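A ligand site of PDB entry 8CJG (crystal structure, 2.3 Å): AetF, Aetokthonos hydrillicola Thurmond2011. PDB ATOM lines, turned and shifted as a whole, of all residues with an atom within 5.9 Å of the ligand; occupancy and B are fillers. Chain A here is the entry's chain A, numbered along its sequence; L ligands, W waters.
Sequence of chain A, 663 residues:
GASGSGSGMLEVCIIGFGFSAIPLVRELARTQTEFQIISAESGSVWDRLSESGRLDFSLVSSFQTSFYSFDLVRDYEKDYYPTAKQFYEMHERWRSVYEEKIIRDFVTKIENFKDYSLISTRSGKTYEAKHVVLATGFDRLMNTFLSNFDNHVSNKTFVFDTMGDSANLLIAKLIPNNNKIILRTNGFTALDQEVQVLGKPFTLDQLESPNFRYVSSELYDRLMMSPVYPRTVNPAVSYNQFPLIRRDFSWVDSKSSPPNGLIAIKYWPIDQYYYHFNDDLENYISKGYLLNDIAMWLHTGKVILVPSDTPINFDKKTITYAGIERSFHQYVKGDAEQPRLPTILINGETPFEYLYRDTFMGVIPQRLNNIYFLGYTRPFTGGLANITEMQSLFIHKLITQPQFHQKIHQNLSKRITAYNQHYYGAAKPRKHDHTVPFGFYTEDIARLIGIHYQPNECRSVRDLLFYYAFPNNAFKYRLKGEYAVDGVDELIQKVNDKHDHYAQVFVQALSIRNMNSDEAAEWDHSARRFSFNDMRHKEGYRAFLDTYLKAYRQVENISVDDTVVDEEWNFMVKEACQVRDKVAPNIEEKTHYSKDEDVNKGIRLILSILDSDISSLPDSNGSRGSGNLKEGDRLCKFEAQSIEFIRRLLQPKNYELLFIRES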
ATOM      1  N   LEU A 191      16.466 -20.565  18.253  1.00  0.00           N
ATOM      2  CA  LEU A 191      15.333 -19.752  17.846  1.00  0.00           C
ATOM      3  C   LEU A 191      14.289 -19.728  18.951  1.00  0.00           C
ATOM      4  O   LEU A 191      13.964 -20.778  19.521  1.00  0.00           O
ATOM      5  CB  LEU A 191      14.708 -20.271  16.549  1.00  0.00           C
ATOM      6  CG  LEU A 191      15.569 -20.231  15.291  1.00  0.00           C
ATOM      7  CD1 LEU A 191      14.888 -20.978  14.154  1.00  0.00           C
ATOM      8  CD2 LEU A 191      15.862 -18.800  14.882  1.00  0.00           C
ATOM      9  N   VAL A 195       7.288 -15.895  19.662  1.00  0.00           N
ATOM     10  CA  VAL A 195       7.725 -14.531  19.430  1.00  0.00           C
ATOM     11  C   VAL A 195       6.502 -13.609  19.541  1.00  0.00           C
ATOM     12  O   VAL A 195       5.365 -14.063  19.666  1.00  0.00           O
ATOM     13  CB  VAL A 195       8.403 -14.355  18.057  1.00  0.00           C
ATOM     14  CG1 VAL A 195       9.418 -15.459  17.814  1.00  0.00           C
ATOM     15  CG2 VAL A 195       7.375 -14.317  16.945  1.00  0.00           C
ATOM     16  N   LEU A 204       6.679 -19.844  16.543  1.00  0.00           N
ATOM     17  CA  LEU A 204       7.492 -19.557  15.359  1.00  0.00           C
ATOM     18  C   LEU A 204       6.984 -20.287  14.122  1.00  0.00           C
ATOM     19  O   LEU A 204       7.135 -19.779  13.005  1.00  0.00           O
ATOM     20  CB  LEU A 204       8.962 -19.902  15.631  1.00  0.00           C
ATOM     21  CG  LEU A 204       9.453 -21.347  15.438  1.00  0.00           C
ATOM     22  CD1 LEU A 204      10.970 -21.379  15.386  1.00  0.00           C
ATOM     23  CD2 LEU A 204       8.940 -22.252  16.534  1.00  0.00           C
ATOM     24  N   ASP A 205       6.361 -21.455  14.299  1.00  0.00           N
ATOM     25  CA  ASP A 205       5.826 -22.191  13.155  1.00  0.00           C
ATOM     26  C   ASP A 205       4.693 -21.459  12.448  1.00  0.00           C
ATOM     27  O   ASP A 205       4.334 -21.819  11.323  1.00  0.00           O
ATOM     28  CB  ASP A 205       5.329 -23.578  13.603  1.00  0.00           C
ATOM     29  CG  ASP A 205       4.346 -23.500  14.751  1.00  0.00           C
ATOM     30  OD1 ASP A 205       4.782 -23.197  15.891  1.00  0.00           O
ATOM     31  OD2 ASP A 205       3.149 -23.739  14.531  1.00  0.00           O
ATOM     32  N   LEU A 207       4.750 -18.293  11.466  1.00  0.00           N
ATOM     33  CA  LEU A 207       5.239 -17.142  10.713  1.00  0.00           C
ATOM     34  C   LEU A 207       6.220 -17.547   9.623  1.00  0.00           C
ATOM     35  O   LEU A 207       7.107 -16.786   9.259  1.00  0.00           O
ATOM     36  CB  LEU A 207       5.899 -16.139  11.669  1.00  0.00           C
ATOM     37  CG  LEU A 207       5.039 -15.680  12.841  1.00  0.00           C
ATOM     38  CD1 LEU A 207       5.838 -14.780  13.751  1.00  0.00           C
ATOM     39  CD2 LEU A 207       3.786 -14.977  12.361  1.00  0.00           C
ATOM     40  N   GLU A 208       6.063 -18.751   9.083  1.00  0.00           N
ATOM     41  CA  GLU A 208       7.000 -19.264   8.097  1.00  0.00           C
ATOM     42  C   GLU A 208       6.507 -19.133   6.662  1.00  0.00           C
ATOM     43  O   GLU A 208       7.333 -19.169   5.742  1.00  0.00           O
ATOM     44  CB  GLU A 208       7.339 -20.734   8.390  1.00  0.00           C
ATOM     45  CG  GLU A 208       7.774 -20.938   9.829  1.00  0.00           C
ATOM     46  CD  GLU A 208       8.451 -22.267  10.067  1.00  0.00           C
ATOM     47  OE1 GLU A 208       8.868 -22.910   9.081  1.00  0.00           O
ATOM     48  OE2 GLU A 208       8.561 -22.675  11.240  1.00  0.00           O
ATOM     49  N   LEU A 223      13.044 -13.662   3.689  1.00  0.00           N
ATOM     50  CA  LEU A 223      11.953 -13.795   4.649  1.00  0.00           C
ATOM     51  C   LEU A 223      12.354 -14.559   5.907  1.00  0.00           C
ATOM     52  O   LEU A 223      11.708 -14.385   6.946  1.00  0.00           O
ATOM     53  CB  LEU A 223      10.766 -14.484   3.982  1.00  0.00           C
ATOM     54  CG  LEU A 223       9.355 -13.923   4.111  1.00  0.00           C
ATOM     55  CD1 LEU A 223       9.357 -12.403   4.022  1.00  0.00           C
ATOM     56  CD2 LEU A 223       8.471 -14.509   3.017  1.00  0.00           C
ATOM     57  N   MET A 224      13.403 -15.372   5.835  1.00  0.00           N
ATOM     58  CA  MET A 224      13.630 -16.388   6.865  1.00  0.00           C
ATOM     59  C   MET A 224      15.046 -16.425   7.419  1.00  0.00           C
ATOM     60  O   MET A 224      15.235 -16.820   8.578  1.00  0.00           O
ATOM     61  CB  MET A 224      13.266 -17.764   6.316  1.00  0.00           C
ATOM     62  CG  MET A 224      11.811 -17.921   5.903  1.00  0.00           C
ATOM     63  SD  MET A 224      10.731 -18.187   7.320  1.00  0.00           S
ATOM     64  CE  MET A 224      11.244 -19.811   7.852  1.00  0.00           C
ATOM     65  N   MET A 225      16.048 -16.046   6.624  1.00  0.00           N
ATOM     66  CA  MET A 225      17.418 -16.466   6.907  1.00  0.00           C
ATOM     67  C   MET A 225      18.252 -15.450   7.673  1.00  0.00           C
ATOM     68  O   MET A 225      19.358 -15.799   8.104  1.00  0.00           O
ATOM     69  CB  MET A 225      18.131 -16.832   5.602  1.00  0.00           C
ATOM     70  CG  MET A 225      17.527 -18.042   4.906  1.00  0.00           C
ATOM     71  SD  MET A 225      17.110 -19.362   6.071  1.00  0.00           S
ATOM     72  CE  MET A 225      18.724 -20.042   6.427  1.00  0.00           C
ATOM     73  N   PRO A 227      17.858 -14.421  10.804  1.00  0.00           N
ATOM     74  CA  PRO A 227      18.180 -14.906  12.150  1.00  0.00           C
ATOM     75  C   PRO A 227      19.124 -16.101  12.184  1.00  0.00           C
ATOM     76  O   PRO A 227      19.559 -16.488  13.277  1.00  0.00           O
ATOM     77  CB  PRO A 227      16.809 -15.288  12.736  1.00  0.00           C
ATOM     78  CG  PRO A 227      15.813 -14.608  11.861  1.00  0.00           C
ATOM     79  CD  PRO A 227      16.420 -14.609  10.514  1.00  0.00           C
ATOM     80  N   VAL A 228      19.433 -16.710  11.044  1.00  0.00           N
ATOM     81  CA  VAL A 228      20.294 -17.883  10.989  1.00  0.00           C
ATOM     82  C   VAL A 228      21.700 -17.520  10.533  1.00  0.00           C
ATOM     83  O   VAL A 228      22.684 -17.906  11.160  1.00  0.00           O
ATOM     84  CB  VAL A 228      19.656 -18.961  10.078  1.00  0.00           C
ATOM     85  CG1 VAL A 228      20.569 -20.179   9.972  1.00  0.00           C
ATOM     86  CG2 VAL A 228      18.288 -19.346  10.595  1.00  0.00           C
ATOM     87  N   PRO A 258      14.958 -22.070   4.125  1.00  0.00           N
ATOM     88  CA  PRO A 258      16.098 -22.664   4.870  1.00  0.00           C
ATOM     89  C   PRO A 258      16.467 -24.040   4.341  1.00  0.00           C
ATOM     90  O   PRO A 258      15.602 -24.831   3.974  1.00  0.00           O
ATOM     91  CB  PRO A 258      15.567 -22.716   6.321  1.00  0.00           C
ATOM     92  CG  PRO A 258      14.073 -22.688   6.204  1.00  0.00           C
ATOM     93  CD  PRO A 258      13.796 -21.831   5.008  1.00  0.00           C
ATOM     94  N   LEU A 262      19.557 -28.191   7.844  1.00  0.00           N
ATOM     95  CA  LEU A 262      19.703 -27.188   8.889  1.00  0.00           C
ATOM     96  C   LEU A 262      18.910 -27.600  10.121  1.00  0.00           C
ATOM     97  O   LEU A 262      17.723 -27.940  10.017  1.00  0.00           O
ATOM     98  CB  LEU A 262      19.227 -25.831   8.384  1.00  0.00           C
ATOM     99  CG  LEU A 262      19.173 -24.652   9.370  1.00  0.00           C
ATOM    100  CD1 LEU A 262      20.565 -24.192   9.733  1.00  0.00           C
ATOM    101  CD2 LEU A 262      18.351 -23.517   8.793  1.00  0.00           C
ATOM    102  N   PHE A 380      12.285 -29.250  10.544  1.00  0.00           N
ATOM    103  CA  PHE A 380      13.155 -28.159  10.971  1.00  0.00           C
ATOM    104  C   PHE A 380      12.523 -27.369  12.111  1.00  0.00           C
ATOM    105  O   PHE A 380      13.192 -27.053  13.100  1.00  0.00           O
ATOM    106  CB  PHE A 380      13.475 -27.262   9.774  1.00  0.00           C
ATOM    107  CG  PHE A 380      14.146 -25.971  10.141  1.00  0.00           C
ATOM    108  CD1 PHE A 380      15.349 -25.968  10.817  1.00  0.00           C
ATOM    109  CD2 PHE A 380      13.581 -24.760   9.770  1.00  0.00           C
ATOM    110  CE1 PHE A 380      15.968 -24.778  11.158  1.00  0.00           C
ATOM    111  CE2 PHE A 380      14.196 -23.568  10.097  1.00  0.00           C
ATOM    112  CZ  PHE A 380      15.397 -23.584  10.784  1.00  0.00           C
ATOM    113  N   THR A 381      11.234 -27.055  11.986  1.00  0.00           N
ATOM    114  CA  THR A 381      10.468 -26.451  13.060  1.00  0.00           C
ATOM    115  C   THR A 381       9.144 -27.185  13.191  1.00  0.00           C
ATOM    116  O   THR A 381       8.709 -27.883  12.264  1.00  0.00           O
ATOM    117  CB  THR A 381      10.214 -24.957  12.829  1.00  0.00           C
ATOM    118  OG1 THR A 381       9.416 -24.784  11.646  1.00  0.00           O
ATOM    119  CG2 THR A 381      11.526 -24.211  12.644  1.00  0.00           C
ATOM    120  N   VAL A 505       2.053 -12.123   8.645  1.00  0.00           N
ATOM    121  CA  VAL A 505       3.204 -12.729   7.969  1.00  0.00           C
ATOM    122  C   VAL A 505       3.114 -12.518   6.473  1.00  0.00           C
ATOM    123  O   VAL A 505       4.132 -12.472   5.775  1.00  0.00           O
ATOM    124  CB  VAL A 505       3.317 -14.226   8.342  1.00  0.00           C
ATOM    125  CG1 VAL A 505       2.170 -15.027   7.752  1.00  0.00           C
ATOM    126  CG2 VAL A 505       4.654 -14.787   7.896  1.00  0.00           C
ATOM    127  N   GLN A 508       4.747  -9.172   5.831  1.00  0.00           N
ATOM    128  CA  GLN A 508       6.205  -9.161   5.853  1.00  0.00           C
ATOM    129  C   GLN A 508       6.785  -9.313   4.463  1.00  0.00           C
ATOM    130  O   GLN A 508       7.737  -8.613   4.093  1.00  0.00           O
ATOM    131  CB  GLN A 508       6.721 -10.274   6.776  1.00  0.00           C
ATOM    132  CG  GLN A 508       8.233 -10.281   6.917  1.00  0.00           C
ATOM    133  CD  GLN A 508       8.743 -11.605   7.451  1.00  0.00           C
ATOM    134  OE1 GLN A 508       7.981 -12.413   7.978  1.00  0.00           O
ATOM    135  NE2 GLN A 508      10.051 -11.827   7.319  1.00  0.00           N
ATOM    136  N   TRP A 523      15.866  -4.597   8.398  1.00  0.00           N
ATOM    137  CA  TRP A 523      14.446  -4.406   8.643  1.00  0.00           C
ATOM    138  C   TRP A 523      13.918  -5.421   9.650  1.00  0.00           C
ATOM    139  O   TRP A 523      13.081  -5.088  10.492  1.00  0.00           O
ATOM    140  CB  TRP A 523      13.681  -4.496   7.312  1.00  0.00           C
ATOM    141  CG  TRP A 523      12.206  -4.287   7.440  1.00  0.00           C
ATOM    142  CD1 TRP A 523      11.532  -3.101   7.316  1.00  0.00           C
ATOM    143  CD2 TRP A 523      11.211  -5.290   7.690  1.00  0.00           C
ATOM    144  NE1 TRP A 523      10.183  -3.312   7.484  1.00  0.00           N
ATOM    145  CE2 TRP A 523       9.960  -4.645   7.715  1.00  0.00           C
ATOM    146  CE3 TRP A 523      11.258  -6.667   7.897  1.00  0.00           C
ATOM    147  CZ2 TRP A 523       8.768  -5.325   7.940  1.00  0.00           C
ATOM    148  CZ3 TRP A 523      10.076  -7.343   8.122  1.00  0.00           C
ATOM    149  CH2 TRP A 523       8.849  -6.680   8.138  1.00  0.00           C
ATOM    150  N   ASP A 524      14.416  -6.662   9.584  1.00  0.00           N
ATOM    151  CA  ASP A 524      13.990  -7.686  10.523  1.00  0.00           C
ATOM    152  C   ASP A 524      14.301  -7.282  11.964  1.00  0.00           C
ATOM    153  O   ASP A 524      13.509  -7.550  12.874  1.00  0.00           O
ATOM    154  CB  ASP A 524      14.663  -9.026  10.203  1.00  0.00           C
ATOM    155  CG  ASP A 524      14.149  -9.636   8.921  1.00  0.00           C
ATOM    156  OD1 ASP A 524      13.028  -9.307   8.489  1.00  0.00           O
ATOM    157  OD2 ASP A 524      14.881 -10.469   8.342  1.00  0.00           O
ATOM    158  N   SER A 531      12.080 -11.091  16.244  1.00  0.00           N
ATOM    159  CA  SER A 531      11.557 -12.420  16.578  1.00  0.00           C
ATOM    160  C   SER A 531      12.533 -13.239  17.403  1.00  0.00           C
ATOM    161  O   SER A 531      12.167 -13.801  18.442  1.00  0.00           O
ATOM    162  CB  SER A 531      11.189 -13.167  15.291  1.00  0.00           C
ATOM    163  OG  SER A 531      10.187 -12.473  14.569  1.00  0.00           O
ATOM    164  N   PHE A 532      13.794 -13.320  16.979  1.00  0.00           N
ATOM    165  CA  PHE A 532      14.711 -14.322  17.501  1.00  0.00           C
ATOM    166  C   PHE A 532      15.958 -13.676  18.093  1.00  0.00           C
ATOM    167  O   PHE A 532      16.595 -12.834  17.445  1.00  0.00           O
ATOM    168  CB  PHE A 532      15.096 -15.326  16.416  1.00  0.00           C
ATOM    169  CG  PHE A 532      13.907 -15.953  15.749  1.00  0.00           C
ATOM    170  CD1 PHE A 532      13.118 -16.865  16.436  1.00  0.00           C
ATOM    171  CD2 PHE A 532      13.581 -15.645  14.445  1.00  0.00           C
ATOM    172  CE1 PHE A 532      12.016 -17.444  15.828  1.00  0.00           C
ATOM    173  CE2 PHE A 532      12.488 -16.221  13.836  1.00  0.00           C
ATOM    174  CZ  PHE A 532      11.708 -17.124  14.530  1.00  0.00           C
ATOM    175  N   LYS A 595      10.043  -2.014  11.252  1.00  0.00           N
ATOM    176  CA  LYS A 595       9.285  -3.244  11.051  1.00  0.00           C
ATOM    177  C   LYS A 595       7.886  -3.152  11.676  1.00  0.00           C
ATOM    178  O   LYS A 595       6.895  -3.543  11.051  1.00  0.00           O
ATOM    179  CB  LYS A 595      10.042  -4.437  11.622  1.00  0.00           C
ATOM    180  CG  LYS A 595       9.187  -5.694  11.739  1.00  0.00           C
ATOM    181  CD  LYS A 595      10.016  -6.961  11.759  1.00  0.00           C
ATOM    182  CE  LYS A 595       9.114  -8.182  11.783  1.00  0.00           C
ATOM    183  NZ  LYS A 595       9.856  -9.436  12.077  1.00  0.00           N
HETATM  184  C1  LIG L   1      10.922 -20.170  11.923  1.00  0.00           C
HETATM  185  C2  LIG L   1      12.929 -19.395  10.899  1.00  0.00           C
HETATM  186  C3  LIG L   1      10.227 -13.345  10.817  1.00  0.00           C
HETATM  187  O1  LIG L   1      10.274 -13.075  12.003  1.00  0.00           O
HETATM  188  C4  LIG L   1       9.223 -14.452  10.297  1.00  0.00           C
HETATM  189  C5  LIG L   1       9.469 -15.741  11.126  1.00  0.00           C
HETATM  190  C6  LIG L   1      10.731 -16.503  10.857  1.00  0.00           C
HETATM  191  C7  LIG L   1      11.872 -15.992  10.263  1.00  0.00           C
HETATM  192  C8  LIG L   1      12.362 -18.138  10.731  1.00  0.00           C
HETATM  193  C9  LIG L   1      11.018 -17.881  11.176  1.00  0.00           C
HETATM  194  C10 LIG L   1      10.331 -18.931  11.764  1.00  0.00           C
HETATM  195  C11 LIG L   1      12.234 -20.424  11.486  1.00  0.00           C
HETATM  196  N1  LIG L   1       9.530 -14.664   8.862  1.00  0.00           N
HETATM  197  N2  LIG L   1      12.857 -16.986  10.186  1.00  0.00           N
HETATM  198  O2  LIG L   1      10.908 -12.843   9.881  1.00  0.00           O
HETATM  199 BR1  LIG L   1      14.730 -19.705  10.277  1.00  0.00          BR
HETATM  200  O   HOH W   1      13.611 -12.793   9.608  1.00  0.00           O
HETATM  201  O   HOH W   2       8.068 -15.962   6.447  1.00  0.00           O
HETATM  202  O   HOH W   3       7.502 -11.007  12.489  1.00  0.00           O
HETATM  203  O   HOH W   4      10.852 -10.269   9.825  1.00  0.00           O
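An oxygen (O1) of the ligand lies within hydrogen-bond range of the side-chain hydroxyl of Ser 531. OE1 of Gln 508 is in hydrogen-bond range of N1 of the ligand (2.9 Å). A nitrogen (N2) of the ligand lies within hydrogen-bond range of the backbone carbonyl oxygen (O) of Met 224 (2.9 Å). A nitrogen (N2) of the ligand lies close to the side-chain sulfur (SD) of Met 224, at 3.8 Å. The backbone carbonyl oxygen (O) of Leu 223 sits at hydrogen-bond distance from a nitrogen (N1) of the ligand (2.9 Å). A nitrogen (N1) of the ligand lies close to the backbone carbonyl oxygen (O) of Leu 207 (3.2 Å). The side-chain amino group (NZ) of Lys 595 is in salt-bridge range of an oxygen (O1) of the ligand (3.7 Å).
The backbone carbonyl oxygen (O) of Leu 223 sits at hydrogen-bond distance from the side-chain amide nitrogen (NE2) of Gln 508, 3.1 Å away. OE1 of Glu 208 lies close to OG1 of Thr 381, at 3.2 Å.
Merely in contact with the ligand: Phe 532 (3.5 Å), Glu 208 (3.5 Å), Leu 204 (3.5 Å), Val 228 (3.6 Å), Leu 191 (3.8 Å) and Phe 380 (3.9 Å). Hydrophobic or aromatic side chains within 4 Å of the ligand: Leu 191, Leu 204, Leu 207, Met 224, Val 228, Phe 380 and Phe 532. The nearest printed residue that does not touch the ligand is Thr 381 (4.02 Å).
Water W4 lies within hydrogen-bond range of an oxygen (O2) of the ligand (2.6 Å), the side-chain amino group of Lys 595 (2.6 Å), the side-chain carboxylate of Asp 524 (2.7 Å) and the side-chain amide nitrogen of Gln 508 (3.1 Å). Water W1 bridges an oxygen (O2) of the ligand and the side-chain carboxylate (OD2) of Asp 524. Water W3 lies within hydrogen-bond range of NZ of Lys 595 and O1 of the ligand.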
